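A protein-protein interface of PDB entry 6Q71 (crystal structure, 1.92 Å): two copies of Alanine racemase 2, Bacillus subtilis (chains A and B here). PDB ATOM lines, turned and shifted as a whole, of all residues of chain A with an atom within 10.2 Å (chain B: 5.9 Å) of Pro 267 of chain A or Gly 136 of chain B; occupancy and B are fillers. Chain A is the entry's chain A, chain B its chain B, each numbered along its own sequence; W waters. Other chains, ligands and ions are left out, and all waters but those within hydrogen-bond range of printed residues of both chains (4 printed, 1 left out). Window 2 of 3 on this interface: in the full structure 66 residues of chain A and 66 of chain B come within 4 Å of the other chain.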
ATOM      1  N   LYS A 261     -26.956  -0.176  -0.342  1.00  0.00           N
ATOM      2  CA  LYS A 261     -27.255  -1.391  -1.077  1.00  0.00           C
ATOM      3  C   LYS A 261     -27.271  -2.601  -0.155  1.00  0.00           C
ATOM      4  O   LYS A 261     -26.635  -2.613   0.909  1.00  0.00           O
ATOM      5  CB  LYS A 261     -26.238  -1.587  -2.197  1.00  0.00           C
ATOM      6  CG  LYS A 261     -24.794  -1.731  -1.695  1.00  0.00           C
ATOM      7  CD  LYS A 261     -23.854  -2.264  -2.800  1.00  0.00           C
ATOM      8  CE  LYS A 261     -22.383  -2.158  -2.382  1.00  0.00           C
ATOM      9  NZ  LYS A 261     -21.805  -0.778  -2.362  1.00  0.00           N
ATOM     10  N   THR A 262     -28.008  -3.613  -0.572  1.00  0.00           N
ATOM     11  CA  THR A 262     -28.003  -4.912   0.100  1.00  0.00           C
ATOM     12  C   THR A 262     -27.088  -5.867  -0.668  1.00  0.00           C
ATOM     13  O   THR A 262     -27.168  -5.950  -1.903  1.00  0.00           O
ATOM     14  CB  THR A 262     -29.437  -5.481   0.201  1.00  0.00           C
ATOM     15  OG1 THR A 262     -30.253  -4.540   0.903  1.00  0.00           O
ATOM     16  CG2 THR A 262     -29.469  -6.831   0.953  1.00  0.00           C
ATOM     17  N   MET A 263     -26.239  -6.597   0.063  1.00  0.00           N
ATOM     18  CA  MET A 263     -25.183  -7.390  -0.558  1.00  0.00           C
ATOM     19  C   MET A 263     -25.680  -8.767  -0.973  1.00  0.00           C
ATOM     20  O   MET A 263     -25.140  -9.811  -0.566  1.00  0.00           O
ATOM     21  CB  MET A 263     -23.991  -7.501   0.384  1.00  0.00           C
ATOM     22  CG  MET A 263     -23.459  -6.119   0.849  1.00  0.00           C
ATOM     23  SD  MET A 263     -22.592  -5.182  -0.454  1.00  0.00           S
ATOM     24  CE  MET A 263     -21.064  -6.112  -0.561  1.00  0.00           C
ATOM     25  N   ARG A 264     -26.692  -8.759  -1.838  1.00  0.00           N
ATOM     26  CA  ARG A 264     -27.354  -9.978  -2.301  1.00  0.00           C
ATOM     27  C   ARG A 264     -26.499 -10.962  -3.081  1.00  0.00           C
ATOM     28  O   ARG A 264     -26.612 -12.159  -2.881  1.00  0.00           O
ATOM     29  CB  ARG A 264     -28.543  -9.603  -3.160  1.00  0.00           C
ATOM     30  CG  ARG A 264     -29.723  -9.257  -2.321  1.00  0.00           C
ATOM     31  CD  ARG A 264     -30.605  -8.233  -2.981  1.00  0.00           C
ATOM     32  NE  ARG A 264     -31.680  -7.838  -2.080  1.00  0.00           N
ATOM     33  CZ  ARG A 264     -32.452  -6.777  -2.265  1.00  0.00           C
ATOM     34  NH1 ARG A 264     -32.265  -5.994  -3.324  1.00  0.00           N
ATOM     35  NH2 ARG A 264     -33.405  -6.498  -1.388  1.00  0.00           N
ATOM     36  N   THR A 265     -25.631 -10.426  -3.908  1.00  0.00           N
ATOM     37  CA  THR A 265     -24.902 -11.277  -4.804  1.00  0.00           C
ATOM     38  C   THR A 265     -23.401 -11.362  -4.491  1.00  0.00           C
ATOM     39  O   THR A 265     -22.899 -10.482  -3.845  1.00  0.00           O
ATOM     40  CB  THR A 265     -25.051 -10.827  -6.269  1.00  0.00           C
ATOM     41  OG1 THR A 265     -24.363  -9.575  -6.453  1.00  0.00           O
ATOM     42  CG2 THR A 265     -26.522 -10.757  -6.680  1.00  0.00           C
ATOM     43  N   GLU A 266     -22.675 -12.359  -5.034  1.00  0.00           N
ATOM     44  CA  GLU A 266     -21.249 -12.619  -4.729  1.00  0.00           C
ATOM     45  C   GLU A 266     -20.370 -11.839  -5.737  1.00  0.00           C
ATOM     46  O   GLU A 266     -20.835 -11.588  -6.811  1.00  0.00           O
ATOM     47  CB  GLU A 266     -20.915 -14.150  -4.658  1.00  0.00           C
ATOM     48  CG  GLU A 266     -22.077 -14.999  -4.040  1.00  0.00           C
ATOM     49  CD  GLU A 266     -21.639 -16.316  -3.367  1.00  0.00           C
ATOM     50  OE1 GLU A 266     -22.465 -17.073  -2.795  1.00  0.00           O
ATOM     51  OE2 GLU A 266     -20.442 -16.593  -3.393  1.00  0.00           O
ATOM     52  N   PRO A 267     -19.121 -11.470  -5.453  1.00  0.00           N
ATOM     53  CA  PRO A 267     -18.467 -11.504  -4.151  1.00  0.00           C
ATOM     54  C   PRO A 267     -19.088 -10.408  -3.204  1.00  0.00           C
ATOM     55  O   PRO A 267     -19.501  -9.419  -3.755  1.00  0.00           O
ATOM     56  CB  PRO A 267     -17.023 -11.257  -4.498  1.00  0.00           C
ATOM     57  CG  PRO A 267     -17.116 -10.355  -5.635  1.00  0.00           C
ATOM     58  CD  PRO A 267     -18.303 -10.745  -6.420  1.00  0.00           C
ATOM     59  N   ARG A 268     -19.112 -10.606  -1.872  1.00  0.00           N
ATOM     60  CA  ARG A 268     -19.660  -9.652  -0.871  1.00  0.00           C
ATOM     61  C   ARG A 268     -18.494  -8.991  -0.195  1.00  0.00           C
ATOM     62  O   ARG A 268     -18.560  -8.536   0.897  1.00  0.00           O
ATOM     63  CB  ARG A 268     -20.627 -10.335   0.107  1.00  0.00           C
ATOM     64  CG  ARG A 268     -21.806 -10.990  -0.598  1.00  0.00           C
ATOM     65  CD  ARG A 268     -22.861 -11.623   0.317  1.00  0.00           C
ATOM     66  NE  ARG A 268     -23.919 -12.287  -0.453  1.00  0.00           N
ATOM     67  CZ  ARG A 268     -23.819 -13.573  -0.898  1.00  0.00           C
ATOM     68  NH1 ARG A 268     -22.682 -14.309  -0.521  1.00  0.00           N
ATOM     69  NH2 ARG A 268     -24.826 -14.136  -1.693  1.00  0.00           N
ATOM     70  N   THR A 269     -17.412  -8.948  -0.925  1.00  0.00           N
ATOM     71  CA  THR A 269     -16.211  -8.335  -0.430  1.00  0.00           C
ATOM     72  C   THR A 269     -16.392  -6.810  -0.327  1.00  0.00           C
ATOM     73  O   THR A 269     -17.045  -6.199  -1.179  1.00  0.00           O
ATOM     74  CB  THR A 269     -15.070  -8.697  -1.379  1.00  0.00           C
ATOM     75  OG1 THR A 269     -15.566  -8.599  -2.729  1.00  0.00           O
ATOM     76  CG2 THR A 269     -14.621 -10.157  -1.118  1.00  0.00           C
ATOM     77  N   VAL A 270     -15.836  -6.203   0.723  1.00  0.00           N
ATOM     78  CA  VAL A 270     -15.913  -4.748   0.897  1.00  0.00           C
ATOM     79  C   VAL A 270     -14.538  -4.078   1.047  1.00  0.00           C
ATOM     80  O   VAL A 270     -13.729  -4.364   1.977  1.00  0.00           O
ATOM     81  CB  VAL A 270     -16.790  -4.380   2.091  1.00  0.00           C
ATOM     82  CG1 VAL A 270     -16.871  -2.830   2.276  1.00  0.00           C
ATOM     83  CG2 VAL A 270     -18.187  -4.996   1.912  1.00  0.00           C
ATOM     84  N   SER A 271     -14.296  -3.202   0.077  1.00  0.00           N
ATOM     85  CA  SER A 271     -13.192  -2.257   0.048  1.00  0.00           C
ATOM     86  C   SER A 271     -11.854  -2.962  -0.155  1.00  0.00           C
ATOM     87  O   SER A 271     -11.816  -4.181  -0.280  1.00  0.00           O
ATOM     88  CB  SER A 271     -13.182  -1.401   1.324  1.00  0.00           C
ATOM     89  OG  SER A 271     -12.360  -0.255   1.119  1.00  0.00           O
ATOM     90  N   TYR A 272     -10.765  -2.195  -0.254  1.00  0.00           N
ATOM     91  CA  TYR A 272      -9.451  -2.781  -0.560  1.00  0.00           C
ATOM     92  C   TYR A 272      -9.048  -3.890   0.392  1.00  0.00           C
ATOM     93  O   TYR A 272      -9.350  -3.849   1.592  1.00  0.00           O
ATOM     94  CB  TYR A 272      -8.365  -1.712  -0.547  1.00  0.00           C
ATOM     95  CG  TYR A 272      -8.451  -0.730  -1.697  1.00  0.00           C
ATOM     96  CD1 TYR A 272      -8.370  -1.162  -3.021  1.00  0.00           C
ATOM     97  CD2 TYR A 272      -8.632   0.617  -1.456  1.00  0.00           C
ATOM     98  CE1 TYR A 272      -8.452  -0.268  -4.057  1.00  0.00           C
ATOM     99  CE2 TYR A 272      -8.720   1.513  -2.475  1.00  0.00           C
ATOM    100  CZ  TYR A 272      -8.619   1.065  -3.772  1.00  0.00           C
ATOM    101  OH  TYR A 272      -8.704   1.964  -4.780  1.00  0.00           O
ATOM    102  N   GLY A 273      -8.350  -4.879  -0.165  1.00  0.00           N
ATOM    103  CA  GLY A 273      -7.892  -6.036   0.577  1.00  0.00           C
ATOM    104  C   GLY A 273      -8.974  -7.058   0.841  1.00  0.00           C
ATOM    105  O   GLY A 273      -8.681  -8.133   1.379  1.00  0.00           O
ATOM    106  N   ALA A 274     -10.218  -6.726   0.499  1.00  0.00           N
ATOM    107  CA  ALA A 274     -11.364  -7.599   0.783  1.00  0.00           C
ATOM    108  C   ALA A 274     -11.317  -8.026   2.252  1.00  0.00           C
ATOM    109  O   ALA A 274     -11.590  -9.170   2.557  1.00  0.00           O
ATOM    110  CB  ALA A 274     -11.386  -8.850  -0.158  1.00  0.00           C
ATOM    111  N   THR A 275     -10.968  -7.106   3.156  1.00  0.00           N
ATOM    112  CA  THR A 275     -10.790  -7.453   4.567  1.00  0.00           C
ATOM    113  C   THR A 275     -12.110  -7.655   5.303  1.00  0.00           C
ATOM    114  O   THR A 275     -12.109  -8.015   6.490  1.00  0.00           O
ATOM    115  CB  THR A 275     -10.009  -6.381   5.346  1.00  0.00           C
ATOM    116  OG1 THR A 275     -10.797  -5.191   5.444  1.00  0.00           O
ATOM    117  CG2 THR A 275      -8.678  -6.089   4.658  1.00  0.00           C
ATOM    118  N   TYR A 276     -13.222  -7.403   4.608  1.00  0.00           N
ATOM    119  CA  TYR A 276     -14.558  -7.524   5.192  1.00  0.00           C
ATOM    120  C   TYR A 276     -15.532  -8.205   4.200  1.00  0.00           C
ATOM    121  O   TYR A 276     -15.594  -7.827   3.033  1.00  0.00           O
ATOM    122  CB  TYR A 276     -15.058  -6.142   5.563  1.00  0.00           C
ATOM    123  CG  TYR A 276     -16.381  -6.114   6.293  1.00  0.00           C
ATOM    124  CD1 TYR A 276     -17.580  -6.171   5.598  1.00  0.00           C
ATOM    125  CD2 TYR A 276     -16.422  -5.997   7.684  1.00  0.00           C
ATOM    126  CE1 TYR A 276     -18.781  -6.139   6.255  1.00  0.00           C
ATOM    127  CE2 TYR A 276     -17.618  -5.944   8.351  1.00  0.00           C
ATOM    128  CZ  TYR A 276     -18.791  -6.020   7.636  1.00  0.00           C
ATOM    129  OH  TYR A 276     -19.973  -5.996   8.316  1.00  0.00           O
ATOM    130  N   ILE A 277     -16.274  -9.213   4.654  1.00  0.00           N
ATOM    131  CA  ILE A 277     -17.235  -9.903   3.794  1.00  0.00           C
ATOM    132  C   ILE A 277     -18.618  -9.756   4.384  1.00  0.00           C
ATOM    133  O   ILE A 277     -18.873 -10.170   5.524  1.00  0.00           O
ATOM    134  CB  ILE A 277     -16.874 -11.394   3.615  1.00  0.00           C
ATOM    135  CG1 ILE A 277     -15.609 -11.515   2.774  1.00  0.00           C
ATOM    136  CG2 ILE A 277     -17.980 -12.168   2.900  1.00  0.00           C
ATOM    137  CD1 ILE A 277     -14.525 -12.271   3.456  1.00  0.00           C
ATOM    138  N   ALA A 278     -19.512  -9.159   3.603  1.00  0.00           N
ATOM    139  CA  ALA A 278     -20.878  -8.889   4.071  1.00  0.00           C
ATOM    140  C   ALA A 278     -21.767 -10.124   4.005  1.00  0.00           C
ATOM    141  O   ALA A 278     -21.518 -11.039   3.201  1.00  0.00           O
ATOM    142  CB  ALA A 278     -21.511  -7.749   3.234  1.00  0.00           C
ATOM    143  N   GLU A 279     -22.799 -10.151   4.847  1.00  0.00           N
ATOM    144  CA  GLU A 279     -23.842 -11.183   4.770  1.00  0.00           C
ATOM    145  C   GLU A 279     -24.735 -10.835   3.592  1.00  0.00           C
ATOM    146  O   GLU A 279     -24.761  -9.659   3.182  1.00  0.00           O
ATOM    147  CB  GLU A 279     -24.677 -11.255   6.067  1.00  0.00           C
ATOM    148  CG  GLU A 279     -23.894 -11.555   7.338  1.00  0.00           C
ATOM    149  CD  GLU A 279     -23.162 -12.869   7.293  1.00  0.00           C
ATOM    150  OE1 GLU A 279     -23.708 -13.840   6.724  1.00  0.00           O
ATOM    151  OE2 GLU A 279     -22.030 -12.918   7.814  1.00  0.00           O
ATOM    152  N   PRO A 280     -25.469 -11.829   3.045  1.00  0.00           N
ATOM    153  CA  PRO A 280     -26.363 -11.644   1.892  1.00  0.00           C
ATOM    154  C   PRO A 280     -27.470 -10.628   2.123  1.00  0.00           C
ATOM    155  O   PRO A 280     -28.013 -10.044   1.186  1.00  0.00           O
ATOM    156  CB  PRO A 280     -26.965 -13.040   1.681  1.00  0.00           C
ATOM    157  CG  PRO A 280     -26.010 -13.960   2.264  1.00  0.00           C
ATOM    158  CD  PRO A 280     -25.435 -13.245   3.454  1.00  0.00           C
ATOM    159  N   ILE A 284     -24.937  -2.114   3.185  1.00  0.00           N
ATOM    160  CA  ILE A 284     -23.714  -1.329   3.200  1.00  0.00           C
ATOM    161  C   ILE A 284     -24.008   0.075   2.661  1.00  0.00           C
ATOM    162  O   ILE A 284     -24.607   0.245   1.592  1.00  0.00           O
ATOM    163  CB  ILE A 284     -22.576  -1.983   2.360  1.00  0.00           C
ATOM    164  CG1 ILE A 284     -22.155  -3.325   2.982  1.00  0.00           C
ATOM    165  CG2 ILE A 284     -21.356  -1.058   2.269  1.00  0.00           C
ATOM    166  CD1 ILE A 284     -21.418  -3.189   4.343  1.00  0.00           C
ATOM    167  N   ALA A 315     -16.837  -0.601   7.757  1.00  0.00           N
ATOM    168  CA  ALA A 315     -16.685  -1.959   7.218  1.00  0.00           C
ATOM    169  C   ALA A 315     -15.567  -1.988   6.176  1.00  0.00           C
ATOM    170  O   ALA A 315     -15.659  -1.306   5.155  1.00  0.00           O
ATOM    171  CB  ALA A 315     -17.991  -2.412   6.616  1.00  0.00           C
ATOM    172  N   GLY A 316     -14.509  -2.752   6.441  1.00  0.00           N
ATOM    173  CA  GLY A 316     -13.383  -2.838   5.525  1.00  0.00           C
ATOM    174  C   GLY A 316     -12.462  -1.631   5.597  1.00  0.00           C
ATOM    175  O   GLY A 316     -12.505  -0.844   6.558  1.00  0.00           O
ATOM    176  N   MET A 324     -16.994   2.840   3.772  1.00  0.00           N
ATOM    177  CA  MET A 324     -18.245   2.100   3.753  1.00  0.00           C
ATOM    178  C   MET A 324     -18.584   1.705   5.202  1.00  0.00           C
ATOM    179  O   MET A 324     -17.687   1.329   5.965  1.00  0.00           O
ATOM    180  CB  MET A 324     -18.093   0.887   2.820  1.00  0.00           C
ATOM    181  CG  MET A 324     -17.938   1.360   1.320  1.00  0.00           C
ATOM    182  SD  MET A 324     -16.398   0.782   0.571  1.00  0.00           S
ATOM    183  CE  MET A 324     -15.212   1.993   1.115  1.00  0.00           C
ATOM    184  N   ASP B 134     -19.751  -2.397 -10.193  1.00  0.00           N
ATOM    185  CA  ASP B 134     -19.155  -2.911  -8.971  1.00  0.00           C
ATOM    186  C   ASP B 134     -19.041  -4.425  -9.125  1.00  0.00           C
ATOM    187  O   ASP B 134     -20.058  -5.126  -9.116  1.00  0.00           O
ATOM    188  CB  ASP B 134     -20.009  -2.521  -7.758  1.00  0.00           C
ATOM    189  CG  ASP B 134     -19.502  -3.091  -6.403  1.00  0.00           C
ATOM    190  OD1 ASP B 134     -18.360  -3.628  -6.269  1.00  0.00           O
ATOM    191  OD2 ASP B 134     -20.306  -2.976  -5.444  1.00  0.00           O
ATOM    192  N   THR B 135     -17.805  -4.897  -9.297  1.00  0.00           N
ATOM    193  CA  THR B 135     -17.515  -6.316  -9.429  1.00  0.00           C
ATOM    194  C   THR B 135     -16.827  -6.906  -8.175  1.00  0.00           C
ATOM    195  O   THR B 135     -16.395  -8.046  -8.190  1.00  0.00           O
ATOM    196  CB  THR B 135     -16.624  -6.585 -10.648  1.00  0.00           C
ATOM    197  OG1 THR B 135     -15.380  -5.899 -10.487  1.00  0.00           O
ATOM    198  CG2 THR B 135     -17.300  -6.142 -11.949  1.00  0.00           C
ATOM    199  N   GLY B 136     -16.731  -6.154  -7.090  1.00  0.00           N
ATOM    200  CA  GLY B 136     -16.191  -6.709  -5.853  1.00  0.00           C
ATOM    201  C   GLY B 136     -15.550  -5.712  -4.888  1.00  0.00           C
ATOM    202  O   GLY B 136     -15.145  -6.077  -3.782  1.00  0.00           O
ATOM    203  N   MET B 137     -15.422  -4.462  -5.308  1.00  0.00           N
ATOM    204  CA  MET B 137     -14.887  -3.452  -4.412  1.00  0.00           C
ATOM    205  C   MET B 137     -15.957  -3.082  -3.363  1.00  0.00           C
ATOM    206  O   MET B 137     -15.623  -2.663  -2.250  1.00  0.00           O
ATOM    207  CB  MET B 137     -14.425  -2.229  -5.202  1.00  0.00           C
ATOM    208  CG  MET B 137     -13.861  -1.092  -4.378  1.00  0.00           C
ATOM    209  SD  MET B 137     -12.266  -1.381  -3.604  1.00  0.00           S
ATOM    210  CE  MET B 137     -12.031   0.261  -2.936  1.00  0.00           C
ATOM    211  N   GLY B 138     -17.226  -3.266  -3.711  1.00  0.00           N
ATOM    212  CA  GLY B 138     -18.328  -3.025  -2.790  1.00  0.00           C
ATOM    213  C   GLY B 138     -18.521  -1.568  -2.351  1.00  0.00           C
ATOM    214  O   GLY B 138     -19.121  -1.298  -1.307  1.00  0.00           O
ATOM    215  N   ARG B 143     -24.346  -3.807  -9.690  1.00  0.00           N
ATOM    216  CA  ARG B 143     -23.803  -5.124  -9.304  1.00  0.00           C
ATOM    217  C   ARG B 143     -24.338  -6.347 -10.079  1.00  0.00           C
ATOM    218  O   ARG B 143     -23.748  -7.432  -9.986  1.00  0.00           O
ATOM    219  CB  ARG B 143     -24.031  -5.351  -7.792  1.00  0.00           C
ATOM    220  CG  ARG B 143     -23.156  -4.420  -6.919  1.00  0.00           C
ATOM    221  CD  ARG B 143     -23.502  -4.482  -5.431  1.00  0.00           C
ATOM    222  NE  ARG B 143     -23.312  -5.826  -4.865  1.00  0.00           N
ATOM    223  CZ  ARG B 143     -22.154  -6.310  -4.417  1.00  0.00           C
ATOM    224  NH1 ARG B 143     -21.047  -5.568  -4.426  1.00  0.00           N
ATOM    225  NH2 ARG B 143     -22.105  -7.551  -3.931  1.00  0.00           N
ATOM    226  N   THR B 168     -14.736  -0.563 -13.961  1.00  0.00           N
ATOM    227  CA  THR B 168     -14.734  -1.179 -12.647  1.00  0.00           C
ATOM    228  C   THR B 168     -13.399  -0.974 -11.933  1.00  0.00           C
ATOM    229  O   THR B 168     -12.411  -0.522 -12.504  1.00  0.00           O
ATOM    230  CB  THR B 168     -15.032  -2.710 -12.734  1.00  0.00           C
ATOM    231  OG1 THR B 168     -15.368  -3.200 -11.437  1.00  0.00           O
ATOM    232  CG2 THR B 168     -13.859  -3.492 -13.298  1.00  0.00           C
ATOM    233  N   HIS B 169     -13.425  -1.273 -10.646  1.00  0.00           N
ATOM    234  CA  HIS B 169     -12.251  -1.136  -9.777  1.00  0.00           C
ATOM    235  C   HIS B 169     -11.895  -2.459  -9.031  1.00  0.00           C
ATOM    236  O   HIS B 169     -12.713  -3.054  -8.473  1.00  0.00           O
ATOM    237  CB  HIS B 169     -12.413   0.070  -8.775  1.00  0.00           C
ATOM    238  CG  HIS B 169     -11.120   0.610  -8.236  1.00  0.00           C
ATOM    239  ND1 HIS B 169     -10.135   1.135  -9.043  1.00  0.00           N
ATOM    240  CD2 HIS B 169     -10.658   0.721  -6.972  1.00  0.00           C
ATOM    241  CE1 HIS B 169      -9.118   1.519  -8.305  1.00  0.00           C
ATOM    242  NE2 HIS B 169      -9.414   1.288  -7.041  1.00  0.00           N
ATOM    243  N   SER B 171     -10.054  -4.617  -6.129  1.00  0.00           N
ATOM    244  CA  SER B 171      -9.857  -4.363  -4.701  1.00  0.00           C
ATOM    245  C   SER B 171      -8.590  -5.018  -4.178  1.00  0.00           C
ATOM    246  O   SER B 171      -8.082  -4.628  -3.113  1.00  0.00           O
ATOM    247  CB  SER B 171     -11.058  -4.858  -3.897  1.00  0.00           C
ATOM    248  OG  SER B 171     -11.025  -6.245  -3.725  1.00  0.00           O
ATOM    249  N   LEU B 180      -9.021 -13.215  -6.538  1.00  0.00           N
ATOM    250  CA  LEU B 180     -10.123 -12.221  -6.531  1.00  0.00           C
ATOM    251  C   LEU B 180     -10.087 -11.339  -7.813  1.00  0.00           C
ATOM    252  O   LEU B 180     -11.054 -11.009  -8.402  1.00  0.00           O
ATOM    253  CB  LEU B 180     -10.176 -11.269  -5.293  1.00  0.00           C
ATOM    254  CG  LEU B 180     -10.524 -11.852  -3.929  1.00  0.00           C
ATOM    255  CD1 LEU B 180     -11.827 -12.652  -3.956  1.00  0.00           C
ATOM    256  CD2 LEU B 180      -9.378 -12.635  -3.297  1.00  0.00           C
ATOM    257  N   GLN B 184     -12.965 -10.780 -10.571  1.00  0.00           N
ATOM    258  CA  GLN B 184     -13.522  -9.466 -10.932  1.00  0.00           C
ATOM    259  C   GLN B 184     -13.459  -9.240 -12.453  1.00  0.00           C
ATOM    260  O   GLN B 184     -14.433  -8.785 -13.087  1.00  0.00           O
ATOM    261  CB  GLN B 184     -12.781  -8.335 -10.203  1.00  0.00           C
ATOM    262  CG  GLN B 184     -13.109  -8.242  -8.724  1.00  0.00           C
ATOM    263  CD  GLN B 184     -12.597  -6.982  -8.074  1.00  0.00           C
ATOM    264  OE1 GLN B 184     -11.532  -6.950  -7.449  1.00  0.00           O
ATOM    265  NE2 GLN B 184     -13.357  -5.923  -8.228  1.00  0.00           N
ATOM    266  N   LYS B 187     -15.930 -11.311 -14.309  1.00  0.00           N
ATOM    267  CA  LYS B 187     -17.273 -10.799 -14.107  1.00  0.00           C
ATOM    268  C   LYS B 187     -17.490  -9.555 -14.947  1.00  0.00           C
ATOM    269  O   LYS B 187     -18.524  -9.427 -15.598  1.00  0.00           O
ATOM    270  CB  LYS B 187     -17.509 -10.488 -12.635  1.00  0.00           C
ATOM    271  CG  LYS B 187     -18.883 -10.017 -12.315  1.00  0.00           C
ATOM    272  CD  LYS B 187     -19.155 -10.021 -10.787  1.00  0.00           C
ATOM    273  CE  LYS B 187     -20.630 -10.326 -10.502  1.00  0.00           C
ATOM    274  NZ  LYS B 187     -20.962 -10.427  -9.047  1.00  0.00           N
HETATM  275  O   HOH W   1     -21.486  -0.874  -5.238  1.00  0.00           O
HETATM  276  O   HOH W   2      -6.237   1.257  -6.122  1.00  0.00           O
HETATM  277  O   HOH W   3     -13.153  -6.013  -1.739  1.00  0.00           O
HETATM  278  O   HOH W   4     -26.122  -7.315  -4.905  1.00  0.00           O
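SD of Met 137 of chain B sits at hydrogen-bond distance from N of Tyr 272 of chain A (3.8 Å). The backbone carbonyl oxygen (O) of Thr 265 of chain A sits at hydrogen-bond distance from the guanidinium group (NH2) of Arg 143 of chain B (3.0 Å). The backbone carbonyl oxygen of Ser 171 of chain B lies within hydrogen-bond range of the backbone NH of Gly 273 of chain A, 3.0 Å away. The side-chain hydroxyl (OH) of Tyr 272 of chain A is in hydrogen-bond range of a ring nitrogen (NE2) of His 169 of chain B (2.5 Å). The side-chain amino group (NZ) of Lys 261 of chain A sits at hydrogen-bond distance from the backbone carbonyl oxygen (O) of Gly 138 of chain B (2.9 Å). The side-chain hydroxyl of Thr 269 of chain A sits at hydrogen-bond distance from the backbone carbonyl oxygen of Gly 136 of chain B (2.8 Å). The backbone carbonyl oxygen (O) of Glu 266 of chain A sits at hydrogen-bond distance from the side-chain amino group (NZ) of Lys 187 of chain B (2.5 Å). The backbone carbonyl oxygen (O) of Pro 267 of chain A lies within hydrogen-bond range of the guanidinium group (NH2) of Arg 143 of chain B, at 3.2 Å. The backbone carbonyl oxygen of Met 137 of chain B is in hydrogen-bond range of the backbone NH of Ser 271 of chain A (2.7 Å).
The backbone NH (N) of Ile 284 of chain A lies within hydrogen-bond range of the backbone carbonyl oxygen (O) of Lys 261 of chain A (2.9 Å). The side-chain carboxylate (OE1) of Glu 266 of chain A is in salt-bridge range of the guanidinium group (NH1) of Arg 268 of chain A (3.6 Å). OD2 of Asp 134 of chain B is in salt-bridge range of NH1 of Arg 143 of chain B (2.9 Å). OD1 of Asp 134 of chain B lies within hydrogen-bond range of N of Met 137 of chain B (3.2 Å). The side-chain amide oxygen (OE1) of Gln 184 of chain B lies within hydrogen-bond range of the backbone NH (N) of Ser 171 of chain B (3.1 Å). The side-chain carboxylate (OD1) of Asp 134 of chain B is in hydrogen-bond range of the backbone NH (N) of Gly 138 of chain B, at 2.8 Å.
Among the printed residues, merely in contact across the chains: Tyr 272 of chain A with Ser 171 of chain B (3.4 Å), Lys 261 of chain A with Arg 143 of chain B (3.5 Å), Pro 267 of chain A with Thr 135 of chain B (3.5 Å), Val 270 of chain A with Met 137 of chain B (3.7 Å), Pro 267 of chain A with Lys 187 of chain B (3.8 Å), Ser 271 of chain A with Ser 171 of chain B (3.8 Å), Pro 267 of chain A with Gly 136 of chain B (3.8 Å), Thr 269 of chain A with Gly 138 of chain B (3.8 Å), Lys 261 of chain A with Asp 134 of chain B (3.8 Å), Met 263 of chain A with Arg 143 of chain B (3.8 Å), Met 324 of chain A with Gly 138 of chain B (3.9 Å) and Thr 269 of chain A with Met 137 of chain B (3.96 Å).
Of the printed residues of chain B, Met 263 of chain A touches Arg 143 (3.8 Å). Of the printed residues of chain B, Thr 269 of chain A touches Gly 136 (2.8 Å), Met 137 (3.96 Å) and Gly 138 (3.8 Å). Printed residues of chain B within 4 Å of Val 270 of chain A: Met 137 (3.7 Å). Ala 278 of chain A touches none of the printed residues of chain B. Of the printed residues of chain A, Gly 138 of chain B touches Lys 261 (2.9 Å), Thr 269 (3.8 Å) and Met 324 (3.9 Å). The nearest residue of chain B that does not touch Pro 267 of chain A is Leu 180 of chain B (5.4 Å).
Hydrophobic or aromatic side chains of chain B within 4 Å of the printed part of chain A: Met 137 and His 169. Along chain B the printed residues that touch a printed residue of chain A span positions 134 to 187. Of the 24 printed residues of chain A, 11 touch a printed residue of chain B. Hydrophobic or aromatic side chains of chain A within 4 Å of the printed part of chain B: Met 263, Pro 267, Tyr 272 and Met 324. Among the printed residues, 21 pairs touch across the chains.
No position is printed for both chains. Of the 21 pairs that touch across the chains among the printed residues, none has its exchanged pair printed and touching as well.
Water W1 lies within hydrogen-bond range of OD2 of Asp 134 of chain B (2.4 Å) and NZ of Lys 261 of chain A (2.9 Å). Water W3 lies within hydrogen-bond range of O of Ser 271 of chain A (2.7 Å), O of Gly 136 of chain B (2.9 Å) and OG of Ser 171 of chain B (2.9 Å). Water W2 lies within hydrogen-bond range of OH of Tyr 272 of chain A (2.9 Å) and NE2 of His 169 of chain B (3.3 Å). Water W4 lies within hydrogen-bond range of NE of Arg 143 of chain B (3.2 Å), OG1 of Thr 265 of chain A (3.3 Å), N of Arg 264 of chain A (3.4 Å) and O of Thr 262 of chain A (3.5 Å).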
